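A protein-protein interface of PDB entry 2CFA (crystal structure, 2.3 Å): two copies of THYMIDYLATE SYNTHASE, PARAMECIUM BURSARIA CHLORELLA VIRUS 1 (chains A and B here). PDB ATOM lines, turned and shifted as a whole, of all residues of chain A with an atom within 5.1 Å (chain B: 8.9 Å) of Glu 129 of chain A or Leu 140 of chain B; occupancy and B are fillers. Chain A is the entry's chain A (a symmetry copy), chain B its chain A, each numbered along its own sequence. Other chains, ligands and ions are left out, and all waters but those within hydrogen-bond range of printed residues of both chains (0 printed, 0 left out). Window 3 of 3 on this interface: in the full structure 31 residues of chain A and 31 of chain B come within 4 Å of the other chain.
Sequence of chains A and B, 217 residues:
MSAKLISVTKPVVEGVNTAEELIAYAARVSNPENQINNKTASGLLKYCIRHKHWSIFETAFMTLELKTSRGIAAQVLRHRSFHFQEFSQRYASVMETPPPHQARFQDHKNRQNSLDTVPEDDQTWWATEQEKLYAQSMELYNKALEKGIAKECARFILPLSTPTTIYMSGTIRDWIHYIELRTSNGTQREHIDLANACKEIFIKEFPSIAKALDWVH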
ATOM      1  N   TRP A 125      22.024  -3.729  14.648  1.00  0.00           N
ATOM      2  CA  TRP A 125      23.224  -3.445  15.435  1.00  0.00           C
ATOM      3  C   TRP A 125      23.170  -2.064  16.108  1.00  0.00           C
ATOM      4  O   TRP A 125      23.755  -1.864  17.178  1.00  0.00           O
ATOM      5  CB  TRP A 125      24.462  -3.586  14.538  1.00  0.00           C
ATOM      6  CG  TRP A 125      25.614  -2.691  14.882  1.00  0.00           C
ATOM      7  CD1 TRP A 125      26.672  -2.991  15.690  1.00  0.00           C
ATOM      8  CD2 TRP A 125      25.828  -1.350  14.419  1.00  0.00           C
ATOM      9  NE1 TRP A 125      27.531  -1.920  15.763  1.00  0.00           N
ATOM     10  CE2 TRP A 125      27.035  -0.899  14.993  1.00  0.00           C
ATOM     11  CE3 TRP A 125      25.114  -0.485  13.577  1.00  0.00           C
ATOM     12  CZ2 TRP A 125      27.549   0.381  14.753  1.00  0.00           C
ATOM     13  CZ3 TRP A 125      25.624   0.787  13.339  1.00  0.00           C
ATOM     14  CH2 TRP A 125      26.829   1.206  13.925  1.00  0.00           C
ATOM     15  N   TRP A 126      22.463  -1.126  15.475  1.00  0.00           N
ATOM     16  CA  TRP A 126      22.322   0.251  15.971  1.00  0.00           C
ATOM     17  C   TRP A 126      21.697   0.330  17.368  1.00  0.00           C
ATOM     18  O   TRP A 126      22.056   1.204  18.162  1.00  0.00           O
ATOM     19  CB  TRP A 126      21.530   1.101  14.962  1.00  0.00           C
ATOM     20  CG  TRP A 126      20.995   2.411  15.499  1.00  0.00           C
ATOM     21  CD1 TRP A 126      19.692   2.702  15.797  1.00  0.00           C
ATOM     22  CD2 TRP A 126      21.746   3.599  15.797  1.00  0.00           C
ATOM     23  NE1 TRP A 126      19.586   3.992  16.258  1.00  0.00           N
ATOM     24  CE2 TRP A 126      20.829   4.566  16.269  1.00  0.00           C
ATOM     25  CE3 TRP A 126      23.103   3.942  15.711  1.00  0.00           C
ATOM     26  CZ2 TRP A 126      21.226   5.853  16.653  1.00  0.00           C
ATOM     27  CZ3 TRP A 126      23.496   5.223  16.098  1.00  0.00           C
ATOM     28  CH2 TRP A 126      22.559   6.159  16.562  1.00  0.00           C
ATOM     29  N   ALA A 127      20.777  -0.587  17.663  1.00  0.00           N
ATOM     30  CA  ALA A 127      20.125  -0.652  18.971  1.00  0.00           C
ATOM     31  C   ALA A 127      21.081  -1.102  20.079  1.00  0.00           C
ATOM     32  O   ALA A 127      20.904  -0.736  21.242  1.00  0.00           O
ATOM     33  CB  ALA A 127      18.910  -1.565  18.913  1.00  0.00           C
ATOM     34  N   THR A 128      22.089  -1.894  19.705  1.00  0.00           N
ATOM     35  CA  THR A 128      23.087  -2.409  20.648  1.00  0.00           C
ATOM     36  C   THR A 128      24.059  -1.315  21.093  1.00  0.00           C
ATOM     37  O   THR A 128      24.358  -1.190  22.285  1.00  0.00           O
ATOM     38  CB  THR A 128      23.893  -3.591  20.043  1.00  0.00           C
ATOM     39  OG1 THR A 128      23.006  -4.484  19.357  1.00  0.00           O
ATOM     40  CG2 THR A 128      24.642  -4.357  21.132  1.00  0.00           C
ATOM     41  N   GLU A 129      24.540  -0.529  20.131  1.00  0.00           N
ATOM     42  CA  GLU A 129      25.536   0.513  20.405  1.00  0.00           C
ATOM     43  C   GLU A 129      24.946   1.826  20.930  1.00  0.00           C
ATOM     44  O   GLU A 129      25.676   2.669  21.455  1.00  0.00           O
ATOM     45  CB  GLU A 129      26.440   0.748  19.191  1.00  0.00           C
ATOM     46  CG  GLU A 129      27.312  -0.454  18.860  1.00  0.00           C
ATOM     47  CD  GLU A 129      28.775  -0.096  18.712  1.00  0.00           C
ATOM     48  OE1 GLU A 129      29.572  -0.521  19.576  1.00  0.00           O
ATOM     49  OE2 GLU A 129      29.130   0.610  17.746  1.00  0.00           O
ATOM     50  N   GLN A 130      23.632   1.989  20.789  1.00  0.00           N
ATOM     51  CA  GLN A 130      22.904   3.062  21.470  1.00  0.00           C
ATOM     52  C   GLN A 130      22.861   2.801  22.972  1.00  0.00           C
ATOM     53  O   GLN A 130      22.925   3.735  23.774  1.00  0.00           O
ATOM     54  CB  GLN A 130      21.477   3.181  20.934  1.00  0.00           C
ATOM     55  CG  GLN A 130      21.300   4.225  19.850  1.00  0.00           C
ATOM     56  CD  GLN A 130      19.841   4.518  19.551  1.00  0.00           C
ATOM     57  OE1 GLN A 130      19.098   3.645  19.100  1.00  0.00           O
ATOM     58  NE2 GLN A 130      19.426   5.758  19.790  1.00  0.00           N
ATOM     59  N   GLU A 131      22.754   1.525  23.335  1.00  0.00           N
ATOM     60  CA  GLU A 131      22.684   1.107  24.731  1.00  0.00           C
ATOM     61  C   GLU A 131      24.019   1.233  25.457  1.00  0.00           C
ATOM     62  O   GLU A 131      24.045   1.540  26.650  1.00  0.00           O
ATOM     63  CB  GLU A 131      22.157  -0.328  24.843  1.00  0.00           C
ATOM     64  CG  GLU A 131      20.648  -0.476  24.623  1.00  0.00           C
ATOM     65  CD  GLU A 131      19.806   0.110  25.754  1.00  0.00           C
ATOM     66  OE1 GLU A 131      20.352   0.381  26.845  1.00  0.00           O
ATOM     67  OE2 GLU A 131      18.587   0.296  25.547  1.00  0.00           O
ATOM     68  N   LYS A 132      25.123   0.995  24.746  1.00  0.00           N
ATOM     69  CA  LYS A 132      26.444   1.074  25.368  1.00  0.00           C
ATOM     70  C   LYS A 132      26.838   2.520  25.661  1.00  0.00           C
ATOM     71  O   LYS A 132      27.224   2.834  26.788  1.00  0.00           O
ATOM     72  CB  LYS A 132      27.527   0.363  24.542  1.00  0.00           C
ATOM     73  CG  LYS A 132      28.682  -0.163  25.408  1.00  0.00           C
ATOM     74  CD  LYS A 132      30.003  -0.283  24.653  1.00  0.00           C
ATOM     75  CE  LYS A 132      30.200  -1.667  24.039  1.00  0.00           C
ATOM     76  NZ  LYS A 132      29.523  -1.808  22.720  1.00  0.00           N
ATOM     77  N   LEU A 133      26.731   3.392  24.657  1.00  0.00           N
ATOM     78  CA  LEU A 133      27.025   4.817  24.840  1.00  0.00           C
ATOM     79  C   LEU A 133      26.186   5.459  25.939  1.00  0.00           C
ATOM     80  O   LEU A 133      26.723   6.166  26.789  1.00  0.00           O
ATOM     81  CB  LEU A 133      26.862   5.600  23.533  1.00  0.00           C
ATOM     82  CG  LEU A 133      28.127   6.049  22.796  1.00  0.00           C
ATOM     83  CD1 LEU A 133      27.762   6.946  21.639  1.00  0.00           C
ATOM     84  CD2 LEU A 133      29.073   6.783  23.716  1.00  0.00           C
ATOM     85  N   LEU B 133      34.127  10.941  25.516  1.00  0.00           N
ATOM     86  CA  LEU B 133      32.732  10.608  25.209  1.00  0.00           C
ATOM     87  C   LEU B 133      32.216  11.310  23.958  1.00  0.00           C
ATOM     88  O   LEU B 133      31.610  10.672  23.100  1.00  0.00           O
ATOM     89  CB  LEU B 133      31.806  10.905  26.394  1.00  0.00           C
ATOM     90  CG  LEU B 133      31.279   9.725  27.214  1.00  0.00           C
ATOM     91  CD1 LEU B 133      30.256  10.205  28.214  1.00  0.00           C
ATOM     92  CD2 LEU B 133      30.654   8.672  26.330  1.00  0.00           C
ATOM     93  N   TYR B 134      32.466  12.616  23.860  1.00  0.00           N
ATOM     94  CA  TYR B 134      32.039  13.414  22.712  1.00  0.00           C
ATOM     95  C   TYR B 134      32.602  12.851  21.409  1.00  0.00           C
ATOM     96  O   TYR B 134      31.854  12.598  20.464  1.00  0.00           O
ATOM     97  CB  TYR B 134      32.450  14.879  22.896  1.00  0.00           C
ATOM     98  CG  TYR B 134      31.955  15.821  21.819  1.00  0.00           C
ATOM     99  CD1 TYR B 134      32.802  16.244  20.796  1.00  0.00           C
ATOM    100  CD2 TYR B 134      30.642  16.300  21.828  1.00  0.00           C
ATOM    101  CE1 TYR B 134      32.357  17.114  19.802  1.00  0.00           C
ATOM    102  CE2 TYR B 134      30.187  17.173  20.840  1.00  0.00           C
ATOM    103  CZ  TYR B 134      31.050  17.573  19.831  1.00  0.00           C
ATOM    104  OH  TYR B 134      30.614  18.432  18.852  1.00  0.00           O
ATOM    105  N   ALA B 135      33.917  12.643  21.376  1.00  0.00           N
ATOM    106  CA  ALA B 135      34.591  12.056  20.218  1.00  0.00           C
ATOM    107  C   ALA B 135      34.057  10.657  19.908  1.00  0.00           C
ATOM    108  O   ALA B 135      33.926  10.282  18.741  1.00  0.00           O
ATOM    109  CB  ALA B 135      36.097  12.015  20.442  1.00  0.00           C
ATOM    110  N   GLN B 136      33.744   9.906  20.962  1.00  0.00           N
ATOM    111  CA  GLN B 136      33.179   8.563  20.842  1.00  0.00           C
ATOM    112  C   GLN B 136      31.717   8.595  20.388  1.00  0.00           C
ATOM    113  O   GLN B 136      31.248   7.664  19.727  1.00  0.00           O
ATOM    114  CB  GLN B 136      33.298   7.826  22.176  1.00  0.00           C
ATOM    115  CG  GLN B 136      33.180   6.317  22.072  1.00  0.00           C
ATOM    116  CD  GLN B 136      32.953   5.656  23.416  1.00  0.00           C
ATOM    117  OE1 GLN B 136      33.456   6.118  24.446  1.00  0.00           O
ATOM    118  NE2 GLN B 136      32.189   4.566  23.416  1.00  0.00           N
ATOM    119  N   SER B 137      31.007   9.663  20.754  1.00  0.00           N
ATOM    120  CA  SER B 137      29.624   9.882  20.321  1.00  0.00           C
ATOM    121  C   SER B 137      29.563  10.309  18.857  1.00  0.00           C
ATOM    122  O   SER B 137      28.665   9.894  18.123  1.00  0.00           O
ATOM    123  CB  SER B 137      28.938  10.930  21.199  1.00  0.00           C
ATOM    124  OG  SER B 137      28.874  10.507  22.548  1.00  0.00           O
ATOM    125  N   MET B 138      30.523  11.137  18.446  1.00  0.00           N
ATOM    126  CA  MET B 138      30.631  11.597  17.061  1.00  0.00           C
ATOM    127  C   MET B 138      31.088  10.486  16.119  1.00  0.00           C
ATOM    128  O   MET B 138      30.730  10.480  14.940  1.00  0.00           O
ATOM    129  CB  MET B 138      31.579  12.796  16.957  1.00  0.00           C
ATOM    130  CG  MET B 138      31.028  14.100  17.539  1.00  0.00           C
ATOM    131  SD  MET B 138      29.415  14.611  16.887  1.00  0.00           S
ATOM    132  CE  MET B 138      29.773  14.834  15.142  1.00  0.00           C
ATOM    133  N   GLU B 139      31.879   9.558  16.654  1.00  0.00           N
ATOM    134  CA  GLU B 139      32.371   8.405  15.903  1.00  0.00           C
ATOM    135  C   GLU B 139      31.207   7.503  15.497  1.00  0.00           C
ATOM    136  O   GLU B 139      31.066   7.157  14.321  1.00  0.00           O
ATOM    137  CB  GLU B 139      33.398   7.623  16.735  1.00  0.00           C
ATOM    138  CG  GLU B 139      34.404   6.801  15.918  1.00  0.00           C
ATOM    139  CD  GLU B 139      33.852   5.463  15.437  1.00  0.00           C
ATOM    140  OE1 GLU B 139      33.259   4.721  16.257  1.00  0.00           O
ATOM    141  OE2 GLU B 139      34.022   5.148  14.238  1.00  0.00           O
ATOM    142  N   LEU B 140      30.380   7.136  16.475  1.00  0.00           N
ATOM    143  CA  LEU B 140      29.187   6.328  16.235  1.00  0.00           C
ATOM    144  C   LEU B 140      28.180   7.061  15.341  1.00  0.00           C
ATOM    145  O   LEU B 140      27.595   6.462  14.438  1.00  0.00           O
ATOM    146  CB  LEU B 140      28.551   5.904  17.565  1.00  0.00           C
ATOM    147  CG  LEU B 140      27.205   5.169  17.624  1.00  0.00           C
ATOM    148  CD1 LEU B 140      27.056   4.072  16.575  1.00  0.00           C
ATOM    149  CD2 LEU B 140      27.013   4.588  19.005  1.00  0.00           C
ATOM    150  N   TYR B 141      27.995   8.356  15.592  1.00  0.00           N
ATOM    151  CA  TYR B 141      27.119   9.189  14.772  1.00  0.00           C
ATOM    152  C   TYR B 141      27.492   9.086  13.291  1.00  0.00           C
ATOM    153  O   TYR B 141      26.632   8.824  12.447  1.00  0.00           O
ATOM    154  CB  TYR B 141      27.163  10.647  15.249  1.00  0.00           C
ATOM    155  CG  TYR B 141      26.354  11.613  14.407  1.00  0.00           C
ATOM    156  CD1 TYR B 141      26.983  12.502  13.537  1.00  0.00           C
ATOM    157  CD2 TYR B 141      24.959  11.636  14.479  1.00  0.00           C
ATOM    158  CE1 TYR B 141      26.245  13.392  12.760  1.00  0.00           C
ATOM    159  CE2 TYR B 141      24.212  12.523  13.709  1.00  0.00           C
ATOM    160  CZ  TYR B 141      24.861  13.396  12.852  1.00  0.00           C
ATOM    161  OH  TYR B 141      24.129  14.274  12.089  1.00  0.00           O
ATOM    162  N   ASN B 142      28.779   9.288  12.995  1.00  0.00           N
ATOM    163  CA  ASN B 142      29.314   9.152  11.639  1.00  0.00           C
ATOM    164  C   ASN B 142      29.084   7.756  11.064  1.00  0.00           C
ATOM    165  O   ASN B 142      28.606   7.617   9.937  1.00  0.00           O
ATOM    166  CB  ASN B 142      30.811   9.491  11.611  1.00  0.00           C
ATOM    167  CG  ASN B 142      31.083  10.988  11.652  1.00  0.00           C
ATOM    168  OD1 ASN B 142      30.167  11.809  11.571  1.00  0.00           O
ATOM    169  ND2 ASN B 142      32.357  11.347  11.770  1.00  0.00           N
ATOM    170  N   LYS B 143      29.421   6.734  11.852  1.00  0.00           N
ATOM    171  CA  LYS B 143      29.240   5.333  11.464  1.00  0.00           C
ATOM    172  C   LYS B 143      27.799   5.040  11.058  1.00  0.00           C
ATOM    173  O   LYS B 143      27.558   4.456  10.002  1.00  0.00           O
ATOM    174  CB  LYS B 143      29.678   4.391  12.594  1.00  0.00           C
ATOM    175  CG  LYS B 143      31.189   4.165  12.685  1.00  0.00           C
ATOM    176  CD  LYS B 143      31.657   2.966  11.848  1.00  0.00           C
ATOM    177  CE  LYS B 143      31.843   1.699  12.693  1.00  0.00           C
ATOM    178  NZ  LYS B 143      30.578   1.167  13.289  1.00  0.00           N
ATOM    179  N   ALA B 144      26.852   5.466  11.895  1.00  0.00           N
ATOM    180  CA  ALA B 144      25.424   5.250  11.652  1.00  0.00           C
ATOM    181  C   ALA B 144      24.951   5.870  10.334  1.00  0.00           C
ATOM    182  O   ALA B 144      24.261   5.213   9.552  1.00  0.00           O
ATOM    183  CB  ALA B 144      24.605   5.774  12.818  1.00  0.00           C
ATOM    184  N   LEU B 145      25.332   7.125  10.092  1.00  0.00           N
ATOM    185  CA  LEU B 145      25.010   7.818   8.842  1.00  0.00           C
ATOM    186  C   LEU B 145      25.627   7.114   7.636  1.00  0.00           C
ATOM    187  O   LEU B 145      24.996   7.007   6.580  1.00  0.00           O
ATOM    188  CB  LEU B 145      25.485   9.274   8.885  1.00  0.00           C
ATOM    189  CG  LEU B 145      24.619  10.337   9.564  1.00  0.00           C
ATOM    190  CD1 LEU B 145      25.373  11.656   9.609  1.00  0.00           C
ATOM    191  CD2 LEU B 145      23.289  10.513   8.842  1.00  0.00           C
ATOM    192  N   GLU B 146      26.861   6.641   7.809  1.00  0.00           N
ATOM    193  CA  GLU B 146      27.577   5.890   6.780  1.00  0.00           C
ATOM    194  C   GLU B 146      26.872   4.570   6.479  1.00  0.00           C
ATOM    195  O   GLU B 146      26.794   4.152   5.321  1.00  0.00           O
ATOM    196  CB  GLU B 146      29.019   5.625   7.221  1.00  0.00           C
ATOM    197  CG  GLU B 146      29.972   5.259   6.088  1.00  0.00           C
ATOM    198  CD  GLU B 146      31.358   4.868   6.580  1.00  0.00           C
ATOM    199  OE1 GLU B 146      31.475   4.303   7.694  1.00  0.00           O
ATOM    200  OE2 GLU B 146      32.334   5.121   5.843  1.00  0.00           O
ATOM    201  N   LYS B 147      26.348   3.933   7.525  1.00  0.00           N
ATOM    202  CA  LYS B 147      25.659   2.650   7.394  1.00  0.00           C
ATOM    203  C   LYS B 147      24.144   2.793   7.171  1.00  0.00           C
ATOM    204  O   LYS B 147      23.363   1.924   7.569  1.00  0.00           O
ATOM    205  CB  LYS B 147      25.967   1.747   8.600  1.00  0.00           C
ATOM    206  CG  LYS B 147      27.461   1.519   8.852  1.00  0.00           C
ATOM    207  CD  LYS B 147      28.142   0.754   7.711  1.00  0.00           C
ATOM    208  CE  LYS B 147      29.602   1.176   7.533  1.00  0.00           C
ATOM    209  NZ  LYS B 147      30.441   0.965   8.751  1.00  0.00           N
ATOM    210  N   ILE B 149      21.660   4.754   8.320  1.00  0.00           N
ATOM    211  CA  ILE B 149      20.726   5.274   9.332  1.00  0.00           C
ATOM    212  C   ILE B 149      20.371   6.745   9.128  1.00  0.00           C
ATOM    213  O   ILE B 149      21.241   7.571   8.837  1.00  0.00           O
ATOM    214  CB  ILE B 149      21.263   5.043  10.740  1.00  0.00           C
ATOM    215  N   ALA B 154      19.922   9.230  14.193  1.00  0.00           N
ATOM    216  CA  ALA B 154      21.305   9.371  14.627  1.00  0.00           C
ATOM    217  C   ALA B 154      21.498  10.571  15.559  1.00  0.00           C
ATOM    218  O   ALA B 154      22.282  10.500  16.508  1.00  0.00           O
ATOM    219  CB  ALA B 154      22.220   9.471  13.419  1.00  0.00           C
ATOM    220  N   ARG B 155      20.771  11.657  15.281  1.00  0.00           N
ATOM    221  CA  ARG B 155      20.755  12.871  16.112  1.00  0.00           C
ATOM    222  C   ARG B 155      20.553  12.631  17.611  1.00  0.00           C
ATOM    223  O   ARG B 155      21.046  13.398  18.436  1.00  0.00           O
ATOM    224  CB  ARG B 155      19.682  13.846  15.612  1.00  0.00           C
ATOM    225  CG  ARG B 155      20.228  15.168  15.092  1.00  0.00           C
ATOM    226  CD  ARG B 155      19.124  16.099  14.563  1.00  0.00           C
ATOM    227  NE  ARG B 155      17.946  16.154  15.435  1.00  0.00           N
ATOM    228  CZ  ARG B 155      17.796  16.969  16.478  1.00  0.00           C
ATOM    229  NH1 ARG B 155      16.678  16.912  17.187  1.00  0.00           N
ATOM    230  NH2 ARG B 155      18.746  17.833  16.822  1.00  0.00           N
ATOM    231  N   ILE B 157      21.792  10.460  19.613  1.00  0.00           N
ATOM    232  CA  ILE B 157      22.965  10.031  20.380  1.00  0.00           C
ATOM    233  C   ILE B 157      23.881  11.219  20.726  1.00  0.00           C
ATOM    234  O   ILE B 157      24.774  11.116  21.570  1.00  0.00           O
ATOM    235  CB  ILE B 157      23.718   8.848  19.683  1.00  0.00           C
ATOM    236  CG1 ILE B 157      24.347   7.931  20.726  1.00  0.00           C
ATOM    237  CG2 ILE B 157      24.749   9.339  18.662  1.00  0.00           C
ATOM    238  CD1 ILE B 157      24.321   6.466  20.341  1.00  0.00           C
ATOM    239  N   LEU B 158      23.619  12.350  20.077  1.00  0.00           N
ATOM    240  CA  LEU B 158      24.351  13.592  20.302  1.00  0.00           C
ATOM    241  C   LEU B 158      24.075  14.170  21.695  1.00  0.00           C
ATOM    242  O   LEU B 158      22.924  14.215  22.127  1.00  0.00           O
ATOM    243  CB  LEU B 158      23.981  14.607  19.216  1.00  0.00           C
ATOM    244  CG  LEU B 158      24.793  14.731  17.913  1.00  0.00           C
ATOM    245  CD1 LEU B 158      25.491  13.446  17.477  1.00  0.00           C
ATOM    246  CD2 LEU B 158      23.903  15.292  16.795  1.00  0.00           C
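O of Trp 125 of chain A lies close to OG1 of Thr 128 of chain A (3.5 Å).
The side-chain amino group (NZ) of Lys 132 of chain A is in salt-bridge range of the side-chain carboxylate (OE1) of Glu 129 of chain A (3.4 Å).
The backbone carbonyl oxygen of Leu 133 of chain B sits at hydrogen-bond distance from the side-chain hydroxyl of Ser 137 of chain B (2.8 Å).
The indole nitrogen of Trp 126 of chain A sits at hydrogen-bond distance from the side-chain amide oxygen of Gln 130 of chain A, 2.9 Å away.
The backbone carbonyl oxygen of Ala 144 of chain B lies within hydrogen-bond range of the backbone NH of Ile 149 of chain B, 2.9 Å away.
Trp 125 of chain A touches Leu 140 of chain B (CH2 to CD1, 3.9 Å).
Leu 140 of chain B touches Trp 126 of chain A (CD1 to CZ3, 3.8 Å).
CH2 of Trp 126 of chain A touches CA of Ala 154 of chain B, at 3.95 Å.
CD2 of Leu 140 of chain B touches O of Glu 129 of chain A, 3.4 Å away.
Ile 157 of chain B touches Gln 130 of chain A (CD1 to CG, 3.8 Å).
CD2 of Leu 133 of chain B touches CD2 of Leu 133 of chain A (3.6 Å).
CD2 of Leu 133 of chain A touches NE2 of Gln 136 of chain B, at 3.8 Å.
CD1 of Leu 133 of chain A touches CA of Ser 137 of chain B, 3.7 Å away.
CD1 of Leu 133 of chain A touches CD2 of Leu 140 of chain B (3.6 Å).
CD1 of Leu 133 of chain A touches CG1 of Ile 157 of chain B (3.7 Å).
Of the printed residues of chain B, Trp 126 of chain A touches Leu 140, Ala 144 and Ala 154.
No residue of chain B comes within 4 Å of Thr 128 of chain A.
Glu 129 of chain A touches just one residue of chain B: Leu 140 (3.4 Å).
Of the printed residues of chain B, Leu 133 of chain A touches Leu 133 (3.6 Å), Gln 136 (3.8 Å), Ser 137 (3.7 Å), Leu 140 (3.6 Å) and Ile 157 (3.7 Å).
Leu 140 of chain B touches four residues of chain A.
Of the printed residues of chain A, Ala 144 of chain B touches Trp 126.
Glu 146 of chain B touches none of the printed residues of chain A.
Ile 149 of chain B touches none of the printed residues of chain A.
Printed residues of chain A within 4 Å of Ala 154 of chain B: Trp 126 (3.95 Å).
Of the printed residues of chain A, Ile 157 of chain B touches Gln 130 and Leu 133.
The nearest printed residue of chain B that does not touch Trp 126 of chain A is Ile 157 of chain B (4.2 Å).
Hydrophobic or aromatic side chains of chain A within 4 Å of the printed part of chain B: Trp 125, Trp 126 and Leu 133.
Along chain A the printed residues that touch a printed residue of chain B span positions 125 to 133.
Of the 20 printed residues of chain B, 8 touch a printed residue of chain A.
Printed residues of chain B that touch a printed residue of chain A: Leu 133, Gln 136, Ser 137, Leu 140, Lys 143, Ala 144, Ala 154 and Ile 157.
Hydrophobic or aromatic side chains of chain B that line the printed part of chain A: Leu 133, Leu 140, Ala 144 and Ile 157.
Among the printed residues, 12 pairs touch across the chains.
Among the printed residues, no Asp or Glu carboxylate lies within 4 Å of a Lys or Arg side-chain nitrogen of the other chain.
Leu 133 of chain B touches its own counterpart, Leu 133 of chain A.
Of the 12 pairs that touch across the chains among the printed residues, 1 has its exchanged pair printed and touching as well.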
